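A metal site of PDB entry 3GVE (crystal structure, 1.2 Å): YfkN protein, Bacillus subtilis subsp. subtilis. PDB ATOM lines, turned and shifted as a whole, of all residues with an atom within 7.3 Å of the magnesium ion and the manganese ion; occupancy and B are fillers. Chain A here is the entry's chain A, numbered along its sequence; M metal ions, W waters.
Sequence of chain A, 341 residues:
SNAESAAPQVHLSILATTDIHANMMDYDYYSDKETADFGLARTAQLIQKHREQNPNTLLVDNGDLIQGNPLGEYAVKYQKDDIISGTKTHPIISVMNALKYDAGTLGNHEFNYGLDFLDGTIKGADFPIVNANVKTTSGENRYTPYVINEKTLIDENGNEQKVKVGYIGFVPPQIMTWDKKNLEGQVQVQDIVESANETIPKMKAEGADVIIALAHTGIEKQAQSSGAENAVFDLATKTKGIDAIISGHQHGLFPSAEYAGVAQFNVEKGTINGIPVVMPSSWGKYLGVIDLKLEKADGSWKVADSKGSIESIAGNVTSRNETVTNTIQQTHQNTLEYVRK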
ATOM      1  N   THR A  18      10.973  20.531   3.244  1.00  0.00           N
ATOM      2  CA  THR A  18      11.897  19.675   3.973  1.00  0.00           C
ATOM      3  C   THR A  18      12.112  20.194   5.385  1.00  0.00           C
ATOM      4  O   THR A  18      12.044  21.379   5.637  1.00  0.00           O
ATOM      5  CB  THR A  18      13.278  19.557   3.245  1.00  0.00           C
ATOM      6  OG1 THR A  18      14.016  18.432   3.754  1.00  0.00           O
ATOM      7  CG2 THR A  18      14.121  20.839   3.397  1.00  0.00           C
ATOM      8  N   ASP A  19      12.426  19.273   6.294  1.00  0.00           N
ATOM      9  CA  ASP A  19      12.816  19.633   7.649  1.00  0.00           C
ATOM     10  C   ASP A  19      11.814  20.590   8.311  1.00  0.00           C
ATOM     11  O   ASP A  19      12.166  21.499   9.026  1.00  0.00           O
ATOM     12  CB  ASP A  19      14.262  20.169   7.677  1.00  0.00           C
ATOM     13  CG  ASP A  19      15.284  19.104   7.309  1.00  0.00           C
ATOM     14  OD1 ASP A  19      15.770  18.414   8.229  1.00  0.00           O
ATOM     15  OD2 ASP A  19      15.577  18.962   6.099  1.00  0.00           O
ATOM     16  N   ILE A  20      10.505  20.305   8.177  1.00  0.00           N
ATOM     17  CA  ILE A  20       9.410  21.127   8.729  1.00  0.00           C
ATOM     18  C   ILE A  20       9.426  21.017  10.245  1.00  0.00           C
ATOM     19  O   ILE A  20       9.118  22.004  10.938  1.00  0.00           O
ATOM     20  CB  ILE A  20       8.050  20.671   8.107  1.00  0.00           C
ATOM     21  CG1 ILE A  20       7.960  21.104   6.675  1.00  0.00           C
ATOM     22  CG2 ILE A  20       6.912  21.259   8.896  1.00  0.00           C
ATOM     23  CD1 ILE A  20       7.927  22.425   6.384  1.00  0.00           C
ATOM     24  N   HIS A  21       9.781  19.857  10.753  1.00  0.00           N
ATOM     25  CA  HIS A  21      10.016  19.576  12.166  1.00  0.00           C
ATOM     26  C   HIS A  21       8.769  19.946  13.000  1.00  0.00           C
ATOM     27  O   HIS A  21       8.865  20.574  14.044  1.00  0.00           O
ATOM     28  CB  HIS A  21      11.287  20.290  12.659  1.00  0.00           C
ATOM     29  CG  HIS A  21      12.552  19.549  12.328  1.00  0.00           C
ATOM     30  ND1 HIS A  21      12.874  18.345  12.901  1.00  0.00           N
ATOM     31  CD2 HIS A  21      13.554  19.837  11.468  1.00  0.00           C
ATOM     32  CE1 HIS A  21      14.025  17.923  12.417  1.00  0.00           C
ATOM     33  NE2 HIS A  21      14.464  18.804  11.535  1.00  0.00           N
ATOM     34  N   ASN A  62      10.238  16.128   2.112  1.00  0.00           N
ATOM     35  CA  ASN A  62      11.522  15.441   2.199  1.00  0.00           C
ATOM     36  C   ASN A  62      11.949  14.899   3.572  1.00  0.00           C
ATOM     37  O   ASN A  62      13.101  14.546   3.744  1.00  0.00           O
ATOM     38  CB  ASN A  62      12.625  16.349   1.643  1.00  0.00           C
ATOM     39  CG  ASN A  62      13.779  15.562   1.031  1.00  0.00           C
ATOM     40  OD1 ASN A  62      13.578  14.568   0.359  1.00  0.00           O
ATOM     41  ND2 ASN A  62      15.017  16.048   1.260  1.00  0.00           N
ATOM     42  N   GLY A  63      11.013  14.817   4.515  1.00  0.00           N
ATOM     43  CA  GLY A  63      11.296  14.224   5.808  1.00  0.00           C
ATOM     44  C   GLY A  63      11.745  15.198   6.892  1.00  0.00           C
ATOM     45  O   GLY A  63      11.825  16.394   6.665  1.00  0.00           O
ATOM     46  N   ASP A  64      12.058  14.654   8.074  1.00  0.00           N
ATOM     47  CA  ASP A  64      12.201  15.436   9.324  1.00  0.00           C
ATOM     48  C   ASP A  64      10.943  16.311   9.493  1.00  0.00           C
ATOM     49  O   ASP A  64      10.999  17.526   9.640  1.00  0.00           O
ATOM     50  CB  ASP A  64      13.504  16.270   9.353  1.00  0.00           C
ATOM     51  CG  ASP A  64      14.664  15.513   9.953  1.00  0.00           C
ATOM     52  OD1 ASP A  64      14.533  14.276  10.125  1.00  0.00           O
ATOM     53  OD2 ASP A  64      15.702  16.166  10.223  1.00  0.00           O
ATOM     54  N   LEU A  65       9.807  15.630   9.458  1.00  0.00           N
ATOM     55  CA  LEU A  65       8.470  16.235   9.416  1.00  0.00           C
ATOM     56  C   LEU A  65       7.689  16.150  10.735  1.00  0.00           C
ATOM     57  O   LEU A  65       7.082  17.111  11.155  1.00  0.00           O
ATOM     58  CB  LEU A  65       7.667  15.577   8.297  1.00  0.00           C
ATOM     59  CG  LEU A  65       6.176  15.905   8.253  1.00  0.00           C
ATOM     60  CD1 LEU A  65       5.965  17.351   7.871  1.00  0.00           C
ATOM     61  CD2 LEU A  65       5.449  14.971   7.258  1.00  0.00           C
ATOM     62  N   GLN A  67       8.590  15.332  13.945  1.00  0.00           N
ATOM     63  CA  GLN A  67       9.271  15.505  15.231  1.00  0.00           C
ATOM     64  C   GLN A  67      10.008  16.830  15.273  1.00  0.00           C
ATOM     65  O   GLN A  67      10.498  17.299  14.273  1.00  0.00           O
ATOM     66  CB  GLN A  67      10.286  14.375  15.415  1.00  0.00           C
ATOM     67  CG  GLN A  67      10.927  14.319  16.798  1.00  0.00           C
ATOM     68  CD  GLN A  67      12.103  15.285  17.004  1.00  0.00           C
ATOM     69  OE1 GLN A  67      12.457  15.603  18.136  1.00  0.00           O
ATOM     70  NE2 GLN A  67      12.709  15.694  15.939  1.00  0.00           N
ATOM     71  N   GLY A 107      12.950  11.161   7.229  1.00  0.00           N
ATOM     72  CA  GLY A 107      14.157  11.810   7.675  1.00  0.00           C
ATOM     73  C   GLY A 107      14.609  11.046   8.946  1.00  0.00           C
ATOM     74  O   GLY A 107      13.940  10.116   9.453  1.00  0.00           O
ATOM     75  N   ASN A 108      15.817  11.409   9.417  1.00  0.00           N
ATOM     76  CA  ASN A 108      16.322  10.694  10.612  1.00  0.00           C
ATOM     77  C   ASN A 108      15.392  10.825  11.812  1.00  0.00           C
ATOM     78  O   ASN A 108      15.213   9.928  12.627  1.00  0.00           O
ATOM     79  CB  ASN A 108      17.767  11.126  10.995  1.00  0.00           C
ATOM     80  CG  ASN A 108      17.992  12.639  10.916  1.00  0.00           C
ATOM     81  OD1 ASN A 108      17.813  13.297   9.897  1.00  0.00           O
ATOM     82  ND2 ASN A 108      18.278  13.195  12.055  1.00  0.00           N
ATOM     83  N   HIS A 109      14.808  12.011  11.964  1.00  0.00           N
ATOM     84  CA  HIS A 109      13.944  12.278  13.154  1.00  0.00           C
ATOM     85  C   HIS A 109      12.619  11.503  13.124  1.00  0.00           C
ATOM     86  O   HIS A 109      11.990  11.413  14.183  1.00  0.00           O
ATOM     87  CB  HIS A 109      13.760  13.774  13.385  1.00  0.00           C
ATOM     88  CG  HIS A 109      15.003  14.394  13.928  1.00  0.00           C
ATOM     89  ND1 HIS A 109      15.419  14.189  15.237  1.00  0.00           N
ATOM     90  CD2 HIS A 109      15.957  15.121  13.315  1.00  0.00           C
ATOM     91  CE1 HIS A 109      16.589  14.824  15.418  1.00  0.00           C
ATOM     92  NE2 HIS A 109      16.921  15.417  14.276  1.00  0.00           N
ATOM     93  N   GLU A 110      12.228  10.939  11.979  1.00  0.00           N
ATOM     94  CA  GLU A 110      11.049  10.086  11.924  1.00  0.00           C
ATOM     95  C   GLU A 110      11.188   8.826  12.777  1.00  0.00           C
ATOM     96  O   GLU A 110      10.205   8.234  13.117  1.00  0.00           O
ATOM     97  CB  GLU A 110      10.724   9.711  10.464  1.00  0.00           C
ATOM     98  CG  GLU A 110       9.621  10.569   9.803  1.00  0.00           C
ATOM     99  CD  GLU A 110      10.066  11.985   9.543  1.00  0.00           C
ATOM    100  OE1 GLU A 110      11.190  12.154   9.054  1.00  0.00           O
ATOM    101  OE2 GLU A 110       9.319  12.904   9.817  1.00  0.00           O
ATOM    102  N   VAL A 171      17.462   7.988   3.484  1.00  0.00           N
ATOM    103  CA  VAL A 171      17.761   8.559   4.800  1.00  0.00           C
ATOM    104  C   VAL A 171      19.225   8.278   5.145  1.00  0.00           C
ATOM    105  O   VAL A 171      19.808   7.344   4.639  1.00  0.00           O
ATOM    106  CB  VAL A 171      16.778   7.989   5.887  1.00  0.00           C
ATOM    107  CG1 VAL A 171      17.139   6.537   6.220  1.00  0.00           C
ATOM    108  CG2 VAL A 171      16.773   8.854   7.148  1.00  0.00           C
ATOM    109  N   PRO A 172      19.842   9.090   5.991  1.00  0.00           N
ATOM    110  CA  PRO A 172      21.263   8.832   6.292  1.00  0.00           C
ATOM    111  C   PRO A 172      21.443   7.547   7.125  1.00  0.00           C
ATOM    112  O   PRO A 172      20.665   7.265   8.013  1.00  0.00           O
ATOM    113  CB  PRO A 172      21.703  10.063   7.105  1.00  0.00           C
ATOM    114  CG  PRO A 172      20.747  11.149   6.654  1.00  0.00           C
ATOM    115  CD  PRO A 172      19.428  10.405   6.518  1.00  0.00           C
ATOM    116  N   TRP A 178      22.192   7.635  15.796  1.00  0.00           N
ATOM    117  CA  TRP A 178      21.273   8.591  16.402  1.00  0.00           C
ATOM    118  C   TRP A 178      20.098   7.925  17.133  1.00  0.00           C
ATOM    119  O   TRP A 178      19.623   8.448  18.121  1.00  0.00           O
ATOM    120  CB  TRP A 178      20.742   9.562  15.339  1.00  0.00           C
ATOM    121  CG  TRP A 178      21.801  10.375  14.663  1.00  0.00           C
ATOM    122  CD1 TRP A 178      22.926  10.883  15.214  1.00  0.00           C
ATOM    123  CD2 TRP A 178      21.793  10.795  13.295  1.00  0.00           C
ATOM    124  NE1 TRP A 178      23.636  11.601  14.285  1.00  0.00           N
ATOM    125  CE2 TRP A 178      22.968  11.546  13.087  1.00  0.00           C
ATOM    126  CE3 TRP A 178      20.935  10.577  12.222  1.00  0.00           C
ATOM    127  CZ2 TRP A 178      23.277  12.107  11.858  1.00  0.00           C
ATOM    128  CZ3 TRP A 178      21.246  11.133  11.005  1.00  0.00           C
ATOM    129  CH2 TRP A 178      22.409  11.890  10.826  1.00  0.00           C
ATOM    130  N   HIS A 216      16.820  12.634   1.786  1.00  0.00           N
ATOM    131  CA  HIS A 216      16.970  13.287   3.081  1.00  0.00           C
ATOM    132  C   HIS A 216      18.430  13.223   3.488  1.00  0.00           C
ATOM    133  O   HIS A 216      18.847  12.385   4.272  1.00  0.00           O
ATOM    134  CB  HIS A 216      16.070  12.757   4.215  1.00  0.00           C
ATOM    135  CG  HIS A 216      16.097  13.646   5.417  1.00  0.00           C
ATOM    136  ND1 HIS A 216      15.263  14.725   5.542  1.00  0.00           N
ATOM    137  CD2 HIS A 216      16.955  13.718   6.467  1.00  0.00           C
ATOM    138  CE1 HIS A 216      15.568  15.399   6.642  1.00  0.00           C
ATOM    139  NE2 HIS A 216      16.590  14.810   7.224  1.00  0.00           N
ATOM    140  N   THR A 217      19.180  14.131   2.901  1.00  0.00           N
ATOM    141  CA  THR A 217      20.631  14.140   2.974  1.00  0.00           C
ATOM    142  C   THR A 217      21.089  15.420   2.284  1.00  0.00           C
ATOM    143  O   THR A 217      20.442  15.886   1.386  1.00  0.00           O
ATOM    144  CB  THR A 217      21.222  12.854   2.314  1.00  0.00           C
ATOM    145  OG1 THR A 217      22.636  12.805   2.510  1.00  0.00           O
ATOM    146  CG2 THR A 217      20.904  12.775   0.816  1.00  0.00           C
ATOM    147  N   GLU A 229      26.997  10.754   5.213  1.00  0.00           N
ATOM    148  CA  GLU A 229      25.808  11.369   5.765  1.00  0.00           C
ATOM    149  C   GLU A 229      25.106  12.288   4.768  1.00  0.00           C
ATOM    150  O   GLU A 229      23.880  12.305   4.685  1.00  0.00           O
ATOM    151  CB  GLU A 229      26.189  12.145   7.028  1.00  0.00           C
ATOM    152  CG  GLU A 229      25.010  12.808   7.755  1.00  0.00           C
ATOM    153  CD  GLU A 229      25.399  13.454   9.085  1.00  0.00           C
ATOM    154  OE1 GLU A 229      26.477  13.138   9.609  1.00  0.00           O
ATOM    155  OE2 GLU A 229      24.615  14.267   9.594  1.00  0.00           O
ATOM    156  N   GLY A 248      17.805  17.935   1.768  1.00  0.00           N
ATOM    157  CA  GLY A 248      17.505  18.483   3.092  1.00  0.00           C
ATOM    158  C   GLY A 248      18.614  18.161   4.077  1.00  0.00           C
ATOM    159  O   GLY A 248      19.780  18.146   3.719  1.00  0.00           O
ATOM    160  N   HIS A 249      18.188  17.887   5.313  1.00  0.00           N
ATOM    161  CA  HIS A 249      19.000  17.430   6.426  1.00  0.00           C
ATOM    162  C   HIS A 249      19.905  18.532   6.995  1.00  0.00           C
ATOM    163  O   HIS A 249      19.928  18.711   8.189  1.00  0.00           O
ATOM    164  CB  HIS A 249      19.786  16.165   6.042  1.00  0.00           C
ATOM    165  CG  HIS A 249      20.553  15.574   7.175  1.00  0.00           C
ATOM    166  ND1 HIS A 249      19.955  15.122   8.330  1.00  0.00           N
ATOM    167  CD2 HIS A 249      21.881  15.349   7.329  1.00  0.00           C
ATOM    168  CE1 HIS A 249      20.877  14.653   9.148  1.00  0.00           C
ATOM    169  NE2 HIS A 249      22.055  14.782   8.560  1.00  0.00           N
ATOM    170  N   GLN A 250      20.645  19.235   6.149  1.00  0.00           N
ATOM    171  CA  GLN A 250      21.607  20.258   6.602  1.00  0.00           C
ATOM    172  C   GLN A 250      20.965  21.571   7.057  1.00  0.00           C
ATOM    173  O   GLN A 250      21.603  22.366   7.719  1.00  0.00           O
ATOM    174  CB  GLN A 250      22.643  20.540   5.513  1.00  0.00           C
ATOM    175  CG  GLN A 250      23.748  19.512   5.426  1.00  0.00           C
ATOM    176  CD  GLN A 250      24.582  19.662   4.164  1.00  0.00           C
ATOM    177  OE1 GLN A 250      24.123  20.158   3.155  1.00  0.00           O
ATOM    178  NE2 GLN A 250      25.806  19.191   4.224  1.00  0.00           N
ATOM    179  N   HIS A 251      19.710  21.781   6.702  1.00  0.00           N
ATOM    180  CA  HIS A 251      19.022  23.034   7.046  1.00  0.00           C
ATOM    181  C   HIS A 251      19.684  24.251   6.343  1.00  0.00           C
ATOM    182  O   HIS A 251      19.564  25.371   6.805  1.00  0.00           O
ATOM    183  CB  HIS A 251      18.941  23.245   8.579  1.00  0.00           C
ATOM    184  CG  HIS A 251      18.098  22.231   9.312  1.00  0.00           C
ATOM    185  ND1 HIS A 251      17.590  22.467  10.566  1.00  0.00           N
ATOM    186  CD2 HIS A 251      17.699  20.971   8.980  1.00  0.00           C
ATOM    187  CE1 HIS A 251      16.883  21.425  10.970  1.00  0.00           C
ATOM    188  NE2 HIS A 251      16.948  20.491  10.036  1.00  0.00           N
ATOM    189  N   SER A 281      15.823  25.122   3.021  1.00  0.00           N
ATOM    190  CA  SER A 281      16.032  25.566   4.394  1.00  0.00           C
ATOM    191  C   SER A 281      15.434  24.554   5.392  1.00  0.00           C
ATOM    192  O   SER A 281      15.615  23.363   5.247  1.00  0.00           O
ATOM    193  CB  SER A 281      15.437  26.985   4.571  1.00  0.00           C
ATOM    194  OG  SER A 281      15.837  27.535   5.818  1.00  0.00           O
ATOM    195  N   SER A 282      14.763  25.062   6.420  1.00  0.00           N
ATOM    196  CA  SER A 282      14.111  24.222   7.417  1.00  0.00           C
ATOM    197  C   SER A 282      12.885  24.961   7.944  1.00  0.00           C
ATOM    198  O   SER A 282      12.728  26.137   7.725  1.00  0.00           O
ATOM    199  CB  SER A 282      15.078  23.867   8.551  1.00  0.00           C
ATOM    200  OG  SER A 282      15.466  25.022   9.247  1.00  0.00           O
ATOM    201  N   TRP A 283      12.003  24.217   8.591  1.00  0.00           N
ATOM    202  CA  TRP A 283      10.833  24.738   9.294  1.00  0.00           C
ATOM    203  C   TRP A 283       9.814  25.460   8.400  1.00  0.00           C
ATOM    204  O   TRP A 283       8.997  26.215   8.884  1.00  0.00           O
ATOM    205  CB  TRP A 283      11.261  25.665  10.455  1.00  0.00           C
ATOM    206  CG  TRP A 283      12.011  24.999  11.560  1.00  0.00           C
ATOM    207  CD1 TRP A 283      12.610  23.790  11.543  1.00  0.00           C
ATOM    208  CD2 TRP A 283      12.233  25.545  12.856  1.00  0.00           C
ATOM    209  NE1 TRP A 283      13.200  23.540  12.766  1.00  0.00           N
ATOM    210  CE2 TRP A 283      12.977  24.602  13.600  1.00  0.00           C
ATOM    211  CE3 TRP A 283      11.876  26.744  13.471  1.00  0.00           C
ATOM    212  CZ2 TRP A 283      13.363  24.824  14.927  1.00  0.00           C
ATOM    213  CZ3 TRP A 283      12.253  26.960  14.789  1.00  0.00           C
ATOM    214  CH2 TRP A 283      12.991  26.001  15.495  1.00  0.00           C
HETATM  215 MG    MG M   1      17.699  15.255   9.208  1.00  0.00          MG
HETATM  216 MN    MN M   2      16.278  18.361  10.321  1.00  0.00          MN
HETATM  217  O   HOH W   1      18.272  17.541   9.848  1.00  0.00           O
HETATM  218  O   HOH W   2      17.204  18.067  12.343  1.00  0.00           O
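NE2 of His 249 lies within hydrogen-bond range of OE2 of Glu 229 (2.8 Å).
O of Asp 19 sits at hydrogen-bond distance from N of Trp 283.
A ring nitrogen (ND1) of His 21 sits at hydrogen-bond distance from the backbone carbonyl oxygen (O) of Gln 67.
The side-chain hydroxyl (OG1) of Thr 18 lies within hydrogen-bond range of the side-chain carboxylate (OD2) of Asp 19 (2.9 Å).
A ring nitrogen (ND1) of His 216 lies within hydrogen-bond range of the backbone carbonyl oxygen of Asn 62.
N of Asp 19 is in hydrogen-bond range of O of Gly 63, 3.0 Å away.
The backbone NH (N) of His 109 lies within hydrogen-bond range of the side-chain carboxylate (OD1) of Asp 64 (2.9 Å).
ND2 of Asn 108 lies close to NE2 of His 109.
Within 4 Å of the magnesium ion: Asp 19, Asp 64, Asn 108, His 216 and His 249.
The nearest printed residue that does not touch the magnesium ion is His 109 (4.5 Å).
Within 4 Å of the manganese ion: Asp 19, His 21, Asp 64 and His 251.
The magnesium ion is bound by the side-chain amide oxygen (OD1) of Asn 108 (2.1 Å), a ring nitrogen (NE2) of His 216 (2.3 Å), the side-chain carboxylate (OD2) of Asp 64 (2.4 Å), a ring nitrogen (ND1) of His 249 (2.4 Å) and water W1 (2.4 Å).
The manganese ion is bound by the side-chain carboxylate of Asp 19 (2.2 Å), water W1 (2.2 Å), a ring nitrogen (NE2) of His 21 (2.2 Å), water W2 (2.2 Å), a ring nitrogen (NE2) of His 251 (2.3 Å) and the side-chain carboxylate of Asp 64 (2.3 Å).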
